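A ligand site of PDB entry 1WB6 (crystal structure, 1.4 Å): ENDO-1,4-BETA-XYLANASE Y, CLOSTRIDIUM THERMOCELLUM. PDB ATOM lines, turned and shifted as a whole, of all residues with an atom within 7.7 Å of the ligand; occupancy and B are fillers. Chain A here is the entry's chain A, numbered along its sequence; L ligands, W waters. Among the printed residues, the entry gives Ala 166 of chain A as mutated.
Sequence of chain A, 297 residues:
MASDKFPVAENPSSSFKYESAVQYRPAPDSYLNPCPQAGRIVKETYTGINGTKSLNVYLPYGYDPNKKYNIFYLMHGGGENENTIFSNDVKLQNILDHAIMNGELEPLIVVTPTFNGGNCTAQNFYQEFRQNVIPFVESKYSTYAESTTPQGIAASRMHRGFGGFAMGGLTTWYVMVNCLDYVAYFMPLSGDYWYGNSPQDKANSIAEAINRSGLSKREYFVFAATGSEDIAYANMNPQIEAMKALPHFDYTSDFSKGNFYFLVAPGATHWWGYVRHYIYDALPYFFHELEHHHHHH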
ATOM      1  N   GLY A  77     -35.504  13.400 -27.143  1.00  0.00           N
ATOM      2  CA  GLY A  77     -35.402  14.852 -27.111  1.00  0.00           C
ATOM      3  C   GLY A  77     -36.593  15.531 -27.744  1.00  0.00           C
ATOM      4  O   GLY A  77     -37.595  14.925 -28.091  1.00  0.00           O
ATOM      5  N   GLY A  78     -36.502  16.844 -27.861  1.00  0.00           N
ATOM      6  CA  GLY A  78     -37.587  17.585 -28.431  1.00  0.00           C
ATOM      7  C   GLY A  78     -37.870  17.212 -29.862  1.00  0.00           C
ATOM      8  O   GLY A  78     -36.956  16.916 -30.645  1.00  0.00           O
ATOM      9  N   PHE A 165     -31.815  12.505 -23.521  1.00  0.00           N
ATOM     10  CA  PHE A 165     -31.097  13.447 -24.379  1.00  0.00           C
ATOM     11  C   PHE A 165     -31.829  14.758 -24.564  1.00  0.00           C
ATOM     12  O   PHE A 165     -33.008  14.745 -24.913  1.00  0.00           O
ATOM     13  CB  PHE A 165     -30.880  12.791 -25.737  1.00  0.00           C
ATOM     14  CG  PHE A 165     -30.354  13.701 -26.815  1.00  0.00           C
ATOM     15  CD1 PHE A 165     -29.166  14.397 -26.660  1.00  0.00           C
ATOM     16  CD2 PHE A 165     -31.021  13.780 -28.011  1.00  0.00           C
ATOM     17  CE1 PHE A 165     -28.729  15.265 -27.676  1.00  0.00           C
ATOM     18  CE2 PHE A 165     -30.533  14.588 -29.038  1.00  0.00           C
ATOM     19  CZ  PHE A 165     -29.408  15.313 -28.841  1.00  0.00           C
ATOM     20  N   ALA A 166     -31.112  15.846 -24.339  1.00  0.00           N
ATOM     21  CA  ALA A 166     -31.570  17.205 -24.719  1.00  0.00           C
ATOM     22  C   ALA A 166     -32.760  17.573 -23.828  1.00  0.00           C
ATOM     23  O   ALA A 166     -32.593  17.582 -22.607  1.00  0.00           O
ATOM     24  CB  ALA A 166     -31.860  17.281 -26.221  1.00  0.00           C
ATOM     25  N   MET A 167     -33.967  17.813 -24.351  1.00  0.00           N
ATOM     26  CA  MET A 167     -35.099  17.977 -23.479  1.00  0.00           C
ATOM     27  C   MET A 167     -35.320  16.728 -22.587  1.00  0.00           C
ATOM     28  O   MET A 167     -35.861  16.838 -21.505  1.00  0.00           O
ATOM     29  CB  MET A 167     -36.343  18.326 -24.248  1.00  0.00           C
ATOM     30  CG  MET A 167     -36.306  19.798 -24.790  1.00  0.00           C
ATOM     31  SD  MET A 167     -35.931  21.044 -23.629  1.00  0.00           S
ATOM     32  CE  MET A 167     -37.297  20.902 -22.551  1.00  0.00           C
ATOM     33  N   GLY A 168     -34.925  15.544 -23.061  1.00  0.00           N
ATOM     34  CA  GLY A 168     -34.928  14.368 -22.215  1.00  0.00           C
ATOM     35  C   GLY A 168     -33.872  14.340 -21.153  1.00  0.00           C
ATOM     36  O   GLY A 168     -34.001  13.580 -20.165  1.00  0.00           O
ATOM     37  N   GLY A 169     -32.800  15.082 -21.339  1.00  0.00           N
ATOM     38  CA  GLY A 169     -31.818  15.360 -20.309  1.00  0.00           C
ATOM     39  C   GLY A 169     -32.446  16.224 -19.218  1.00  0.00           C
ATOM     40  O   GLY A 169     -32.282  15.964 -18.034  1.00  0.00           O
ATOM     41  N   LEU A 170     -33.154  17.275 -19.612  1.00  0.00           N
ATOM     42  CA  LEU A 170     -33.989  18.024 -18.678  1.00  0.00           C
ATOM     43  C   LEU A 170     -34.947  17.090 -17.919  1.00  0.00           C
ATOM     44  O   LEU A 170     -35.061  17.174 -16.697  1.00  0.00           O
ATOM     45  CB  LEU A 170     -34.713  19.177 -19.411  1.00  0.00           C
ATOM     46  CG  LEU A 170     -35.615  20.041 -18.511  1.00  0.00           C
ATOM     47  CD1 LEU A 170     -35.634  21.457 -18.906  1.00  0.00           C
ATOM     48  CD2 LEU A 170     -36.960  19.482 -18.419  1.00  0.00           C
ATOM     49  N   THR A 171     -35.615  16.194 -18.647  1.00  0.00           N
ATOM     50  CA  THR A 171     -36.499  15.242 -17.968  1.00  0.00           C
ATOM     51  C   THR A 171     -35.766  14.495 -16.882  1.00  0.00           C
ATOM     52  O   THR A 171     -36.268  14.341 -15.764  1.00  0.00           O
ATOM     53  CB  THR A 171     -37.095  14.239 -18.943  1.00  0.00           C
ATOM     54  OG1 THR A 171     -37.841  14.925 -19.958  1.00  0.00           O
ATOM     55  CG2 THR A 171     -37.982  13.207 -18.284  1.00  0.00           C
ATOM     56  N   TRP A 173     -33.123  15.337 -15.107  1.00  0.00           N
ATOM     57  CA  TRP A 173     -32.843  16.143 -13.908  1.00  0.00           C
ATOM     58  C   TRP A 173     -34.087  16.302 -13.043  1.00  0.00           C
ATOM     59  O   TRP A 173     -34.001  16.230 -11.822  1.00  0.00           O
ATOM     60  CB  TRP A 173     -32.292  17.516 -14.273  1.00  0.00           C
ATOM     61  CG  TRP A 173     -30.930  17.518 -14.912  1.00  0.00           C
ATOM     62  CD1 TRP A 173     -30.635  17.890 -16.179  1.00  0.00           C
ATOM     63  CD2 TRP A 173     -29.662  17.224 -14.286  1.00  0.00           C
ATOM     64  NE1 TRP A 173     -29.289  17.806 -16.406  1.00  0.00           N
ATOM     65  CE2 TRP A 173     -28.660  17.392 -15.260  1.00  0.00           C
ATOM     66  CE3 TRP A 173     -29.295  16.782 -13.033  1.00  0.00           C
ATOM     67  CZ2 TRP A 173     -27.293  17.191 -14.968  1.00  0.00           C
ATOM     68  CZ3 TRP A 173     -27.971  16.583 -12.733  1.00  0.00           C
ATOM     69  CH2 TRP A 173     -26.992  16.765 -13.692  1.00  0.00           C
ATOM     70  N   LEU A 189     -27.964  13.558 -20.638  1.00  0.00           N
ATOM     71  CA  LEU A 189     -27.178  13.671 -21.859  1.00  0.00           C
ATOM     72  C   LEU A 189     -27.525  14.977 -22.566  1.00  0.00           C
ATOM     73  O   LEU A 189     -28.680  15.173 -22.976  1.00  0.00           O
ATOM     74  CB  LEU A 189     -27.467  12.506 -22.809  1.00  0.00           C
ATOM     75  CG  LEU A 189     -27.235  11.134 -22.186  1.00  0.00           C
ATOM     76  CD1 LEU A 189     -27.894  10.065 -23.049  1.00  0.00           C
ATOM     77  CD2 LEU A 189     -25.747  10.840 -21.942  1.00  0.00           C
ATOM     78  N   SER A 190     -26.547  15.885 -22.657  1.00  0.00           N
ATOM     79  CA  SER A 190     -26.772  17.122 -23.429  1.00  0.00           C
ATOM     80  C   SER A 190     -28.056  17.875 -23.037  1.00  0.00           C
ATOM     81  O   SER A 190     -28.800  18.369 -23.888  1.00  0.00           O
ATOM     82  CB  SER A 190     -26.752  16.843 -24.938  1.00  0.00           C
ATOM     83  OG  SER A 190     -25.498  16.300 -25.300  1.00  0.00           O
ATOM     84  N   GLY A 191     -28.232  18.075 -21.766  1.00  0.00           N
ATOM     85  CA  GLY A 191     -29.290  18.911 -21.226  1.00  0.00           C
ATOM     86  C   GLY A 191     -28.958  19.259 -19.795  1.00  0.00           C
ATOM     87  O   GLY A 191     -28.428  18.454 -19.050  1.00  0.00           O
ATOM     88  N   ASP A 192     -29.281  20.506 -19.400  1.00  0.00           N
ATOM     89  CA  ASP A 192     -29.130  20.955 -18.053  1.00  0.00           C
ATOM     90  C   ASP A 192     -30.481  21.004 -17.310  1.00  0.00           C
ATOM     91  O   ASP A 192     -31.538  20.798 -17.900  1.00  0.00           O
ATOM     92  CB  ASP A 192     -28.441  22.347 -18.034  1.00  0.00           C
ATOM     93  CG  ASP A 192     -29.275  23.459 -18.657  1.00  0.00           C
ATOM     94  OD1 ASP A 192     -29.682  23.308 -19.849  1.00  0.00           O
ATOM     95  OD2 ASP A 192     -29.530  24.512 -17.998  1.00  0.00           O
ATOM     96  N   TYR A 193     -30.391  21.254 -16.017  1.00  0.00           N
ATOM     97  CA  TYR A 193     -31.540  21.334 -15.111  1.00  0.00           C
ATOM     98  C   TYR A 193     -32.066  22.772 -15.083  1.00  0.00           C
ATOM     99  O   TYR A 193     -31.354  23.676 -14.631  1.00  0.00           O
ATOM    100  CB  TYR A 193     -31.101  20.901 -13.722  1.00  0.00           C
ATOM    101  CG  TYR A 193     -32.113  20.956 -12.607  1.00  0.00           C
ATOM    102  CD1 TYR A 193     -33.467  20.602 -12.798  1.00  0.00           C
ATOM    103  CD2 TYR A 193     -31.700  21.277 -11.321  1.00  0.00           C
ATOM    104  CE1 TYR A 193     -34.362  20.628 -11.724  1.00  0.00           C
ATOM    105  CE2 TYR A 193     -32.597  21.270 -10.274  1.00  0.00           C
ATOM    106  CZ  TYR A 193     -33.901  20.949 -10.453  1.00  0.00           C
ATOM    107  OH  TYR A 193     -34.842  20.958  -9.433  1.00  0.00           O
ATOM    108  N   TRP A 194     -33.299  23.017 -15.506  1.00  0.00           N
ATOM    109  CA  TRP A 194     -33.785  24.413 -15.684  1.00  0.00           C
ATOM    110  C   TRP A 194     -34.316  25.123 -14.382  1.00  0.00           C
ATOM    111  O   TRP A 194     -34.754  26.291 -14.415  1.00  0.00           O
ATOM    112  CB  TRP A 194     -34.741  24.511 -16.906  1.00  0.00           C
ATOM    113  CG  TRP A 194     -34.067  24.421 -18.194  1.00  0.00           C
ATOM    114  CD1 TRP A 194     -32.743  24.099 -18.448  1.00  0.00           C
ATOM    115  CD2 TRP A 194     -34.674  24.545 -19.472  1.00  0.00           C
ATOM    116  NE1 TRP A 194     -32.500  24.056 -19.794  1.00  0.00           N
ATOM    117  CE2 TRP A 194     -33.677  24.298 -20.448  1.00  0.00           C
ATOM    118  CE3 TRP A 194     -35.954  24.861 -19.903  1.00  0.00           C
ATOM    119  CZ2 TRP A 194     -33.922  24.353 -21.808  1.00  0.00           C
ATOM    120  CZ3 TRP A 194     -36.209  24.871 -21.234  1.00  0.00           C
ATOM    121  CH2 TRP A 194     -35.214  24.633 -22.184  1.00  0.00           C
ATOM    122  N   LYS A 202     -29.307  25.722  -9.115  1.00  0.00           N
ATOM    123  CA  LYS A 202     -29.542  24.352  -9.632  1.00  0.00           C
ATOM    124  C   LYS A 202     -28.912  23.318  -8.705  1.00  0.00           C
ATOM    125  O   LYS A 202     -29.559  22.326  -8.333  1.00  0.00           O
ATOM    126  CB  LYS A 202     -28.980  24.242 -11.051  1.00  0.00           C
ATOM    127  CG  LYS A 202     -29.629  25.135 -12.047  1.00  0.00           C
ATOM    128  CD  LYS A 202     -28.946  25.095 -13.389  1.00  0.00           C
ATOM    129  CE  LYS A 202     -29.528  26.143 -14.367  1.00  0.00           C
ATOM    130  NZ  LYS A 202     -28.988  25.987 -15.729  1.00  0.00           N
ATOM    131  N   ASP A 230     -21.305  20.462 -28.602  1.00  0.00           N
ATOM    132  CA  ASP A 230     -22.729  20.359 -28.399  1.00  0.00           C
ATOM    133  C   ASP A 230     -23.201  21.588 -27.628  1.00  0.00           C
ATOM    134  O   ASP A 230     -22.662  21.863 -26.564  1.00  0.00           O
ATOM    135  CB  ASP A 230     -22.988  19.070 -27.590  1.00  0.00           C
ATOM    136  CG  ASP A 230     -24.436  18.734 -27.401  1.00  0.00           C
ATOM    137  OD1 ASP A 230     -25.306  19.624 -27.130  1.00  0.00           O
ATOM    138  OD2 ASP A 230     -24.785  17.515 -27.556  1.00  0.00           O
ATOM    139  N   ILE A 231     -24.183  22.314 -28.178  1.00  0.00           N
ATOM    140  CA  ILE A 231     -24.687  23.515 -27.545  1.00  0.00           C
ATOM    141  C   ILE A 231     -25.047  23.351 -26.078  1.00  0.00           C
ATOM    142  O   ILE A 231     -24.933  24.275 -25.283  1.00  0.00           O
ATOM    143  CB  ILE A 231     -25.871  24.086 -28.343  1.00  0.00           C
ATOM    144  CG1 ILE A 231     -26.958  23.028 -28.572  1.00  0.00           C
ATOM    145  CG2 ILE A 231     -25.362  24.712 -29.644  1.00  0.00           C
ATOM    146  CD1 ILE A 231     -28.243  23.478 -29.178  1.00  0.00           C
ATOM    147  N   ALA A 232     -25.447  22.149 -25.667  1.00  0.00           N
ATOM    148  CA  ALA A 232     -25.814  21.937 -24.275  1.00  0.00           C
ATOM    149  C   ALA A 232     -24.656  22.099 -23.301  1.00  0.00           C
ATOM    150  O   ALA A 232     -24.892  22.345 -22.122  1.00  0.00           O
ATOM    151  CB  ALA A 232     -26.419  20.495 -24.106  1.00  0.00           C
ATOM    152  N   TYR A 233     -23.423  21.975 -23.757  1.00  0.00           N
ATOM    153  CA  TYR A 233     -22.271  22.212 -22.914  1.00  0.00           C
ATOM    154  C   TYR A 233     -22.324  23.568 -22.201  1.00  0.00           C
ATOM    155  O   TYR A 233     -21.898  23.681 -21.060  1.00  0.00           O
ATOM    156  CB  TYR A 233     -20.993  22.048 -23.742  1.00  0.00           C
ATOM    157  CG  TYR A 233     -19.705  22.316 -22.996  1.00  0.00           C
ATOM    158  CD1 TYR A 233     -19.200  23.610 -22.866  1.00  0.00           C
ATOM    159  CD2 TYR A 233     -19.008  21.298 -22.350  1.00  0.00           C
ATOM    160  CE1 TYR A 233     -18.077  23.860 -22.183  1.00  0.00           C
ATOM    161  CE2 TYR A 233     -17.846  21.555 -21.649  1.00  0.00           C
ATOM    162  CZ  TYR A 233     -17.375  22.850 -21.569  1.00  0.00           C
ATOM    163  OH  TYR A 233     -16.220  23.113 -20.871  1.00  0.00           O
ATOM    164  N   ALA A 234     -22.791  24.571 -22.928  1.00  0.00           N
ATOM    165  CA  ALA A 234     -22.787  25.927 -22.379  1.00  0.00           C
ATOM    166  C   ALA A 234     -23.490  26.023 -21.044  1.00  0.00           C
ATOM    167  O   ALA A 234     -23.043  26.732 -20.134  1.00  0.00           O
ATOM    168  CB  ALA A 234     -23.426  26.876 -23.385  1.00  0.00           C
ATOM    169  N   ASN A 235     -24.640  25.343 -20.906  1.00  0.00           N
ATOM    170  CA  ASN A 235     -25.404  25.376 -19.679  1.00  0.00           C
ATOM    171  C   ASN A 235     -25.061  24.199 -18.744  1.00  0.00           C
ATOM    172  O   ASN A 235     -25.126  24.330 -17.546  1.00  0.00           O
ATOM    173  CB  ASN A 235     -26.899  25.357 -20.005  1.00  0.00           C
ATOM    174  CG  ASN A 235     -27.357  26.581 -20.708  1.00  0.00           C
ATOM    175  OD1 ASN A 235     -27.003  27.649 -20.319  1.00  0.00           O
ATOM    176  ND2 ASN A 235     -28.192  26.406 -21.721  1.00  0.00           N
ATOM    177  N   MET A 236     -24.657  23.048 -19.303  1.00  0.00           N
ATOM    178  CA  MET A 236     -24.256  21.946 -18.453  1.00  0.00           C
ATOM    179  C   MET A 236     -23.018  22.238 -17.670  1.00  0.00           C
ATOM    180  O   MET A 236     -22.953  21.923 -16.489  1.00  0.00           O
ATOM    181  CB  MET A 236     -24.082  20.624 -19.221  1.00  0.00           C
ATOM    182  CG  MET A 236     -25.348  20.015 -19.727  1.00  0.00           C
ATOM    183  SD  MET A 236     -25.016  18.392 -20.490  1.00  0.00           S
ATOM    184  CE  MET A 236     -25.084  17.317 -19.107  1.00  0.00           C
ATOM    185  N   HIS A 270     -24.548  18.141 -31.311  1.00  0.00           N
ATOM    186  CA  HIS A 270     -25.840  17.773 -30.718  1.00  0.00           C
ATOM    187  C   HIS A 270     -26.632  16.954 -31.679  1.00  0.00           C
ATOM    188  O   HIS A 270     -27.496  17.405 -32.427  1.00  0.00           O
ATOM    189  CB  HIS A 270     -26.527  19.018 -30.308  1.00  0.00           C
ATOM    190  CG  HIS A 270     -27.837  18.923 -29.653  1.00  0.00           C
ATOM    191  ND1 HIS A 270     -27.913  19.236 -28.331  1.00  0.00           N
ATOM    192  CD2 HIS A 270     -29.032  18.437 -29.957  1.00  0.00           C
ATOM    193  CE1 HIS A 270     -29.230  19.469 -28.105  1.00  0.00           C
ATOM    194  NE2 HIS A 270     -29.899  18.794 -28.946  1.00  0.00           N
HETATM  195  C1  LIG L   1     -31.192  21.916 -25.502  1.00  0.00           C
HETATM  196  C2  LIG L   1     -30.030  22.670 -25.747  1.00  0.00           C
HETATM  197  C3  LIG L   1     -31.562  21.571 -24.201  1.00  0.00           C
HETATM  198  C4  LIG L   1     -29.231  23.124 -24.684  1.00  0.00           C
HETATM  199  C5  LIG L   1     -30.764  22.004 -23.146  1.00  0.00           C
HETATM  200  O1  LIG L   1     -31.030  21.721 -21.836  1.00  0.00           O
HETATM  201  C6  LIG L   1     -29.580  22.790 -23.376  1.00  0.00           C
HETATM  202  C7  LIG L   1     -32.007  21.492 -26.631  1.00  0.00           C
HETATM  203  C8  LIG L   1     -32.227  21.003 -21.473  1.00  0.00           C
HETATM  204  O2  LIG L   1     -33.023  20.850 -26.508  1.00  0.00           O
HETATM  205  O3  LIG L   1     -31.559  21.969 -27.889  1.00  0.00           O
HETATM  206  O4  LIG L   1     -28.855  23.174 -22.277  1.00  0.00           O
HETATM  207  C9  LIG L   1     -32.357  21.722 -29.031  1.00  0.00           C
HETATM  208  O   HOH W   1     -35.940  20.921 -28.106  1.00  0.00           O
HETATM  209  O   HOH W   2     -33.553  24.358 -26.659  1.00  0.00           O
HETATM  210  O   HOH W   3     -34.449  18.598 -27.344  1.00  0.00           O
HETATM  211  O   HOH W   4     -26.542  25.116 -23.174  1.00  0.00           O
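N of Asp 192 lies within hydrogen-bond range of O1 of the ligand (3.2 Å).
An oxygen (O4) of the ligand sits at hydrogen-bond distance from the side-chain carboxylate of Asp 192 (2.6 Å).
ND2 of Asn 235 is in hydrogen-bond range of O4 of the ligand, 3.3 Å away.
NE1 of Trp 194 lies within hydrogen-bond range of O1 of the ligand (3.4 Å).
The indole nitrogen (NE1) of Trp 194 lies within hydrogen-bond range of the side-chain carboxylate (OD1) of Asp 192 (2.9 Å).
The backbone NH (N) of Gly 191 lies within hydrogen-bond range of the side-chain sulfur (SD) of Met 236.
The backbone carbonyl oxygen (O) of Gly 191 sits at hydrogen-bond distance from the indole nitrogen (NE1) of Trp 173.
OD1 of Asp 230 lies within hydrogen-bond range of ND1 of His 270, at 2.9 Å.
The backbone NH (N) of Ala 166 lies close to the backbone carbonyl oxygen (O) of Ser 190 (3.5 Å).
N of Ala 166 lies within hydrogen-bond range of O of Leu 189.
The backbone NH (N) of Ala 232 is in hydrogen-bond range of the side-chain carboxylate (OD1) of Asp 230.
The backbone carbonyl oxygen (O) of Met 167 sits at hydrogen-bond distance from the side-chain hydroxyl (OG1) of Thr 171 (3.2 Å).
Ala 166 touches the ligand.
N of Met 167 touches O2 of the ligand, at 3.8 Å.
CB of Leu 170 touches C8 of the ligand, 3.7 Å away.
Gly 191 touches the ligand (CA to O1, 3.4 Å).
Ile 231 touches the ligand (CD1 to O3, 3.9 Å).
Ala 232 touches the ligand (CA to C4, 3.6 Å).
CE1 of His 270 touches O3 of the ligand (3.4 Å).
Hydrophobic or aromatic side chains within 4 Å of the ligand: Ala 166, Met 167, Leu 170, Trp 194, Ile 231, Ala 232 and His 270.
Within 4 Å of the ligand: Ala 166, Met 167, Leu 170, Gly 191, Asp 192, Trp 194, Ile 231, Ala 232, Asn 235 and His 270.
Water W3 lies within hydrogen-bond range of the backbone NH of Gly 78 (2.7 Å), an oxygen (O2) of the ligand (2.8 Å) and the backbone NH of Met 167 (3.1 Å).
Water W4 lies within hydrogen-bond range of the side-chain amide nitrogen (ND2) of Asn 235, the backbone carbonyl oxygen (O) of Ile 231, an oxygen (O4) of the ligand and the backbone carbonyl oxygen (O) of Ala 232.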
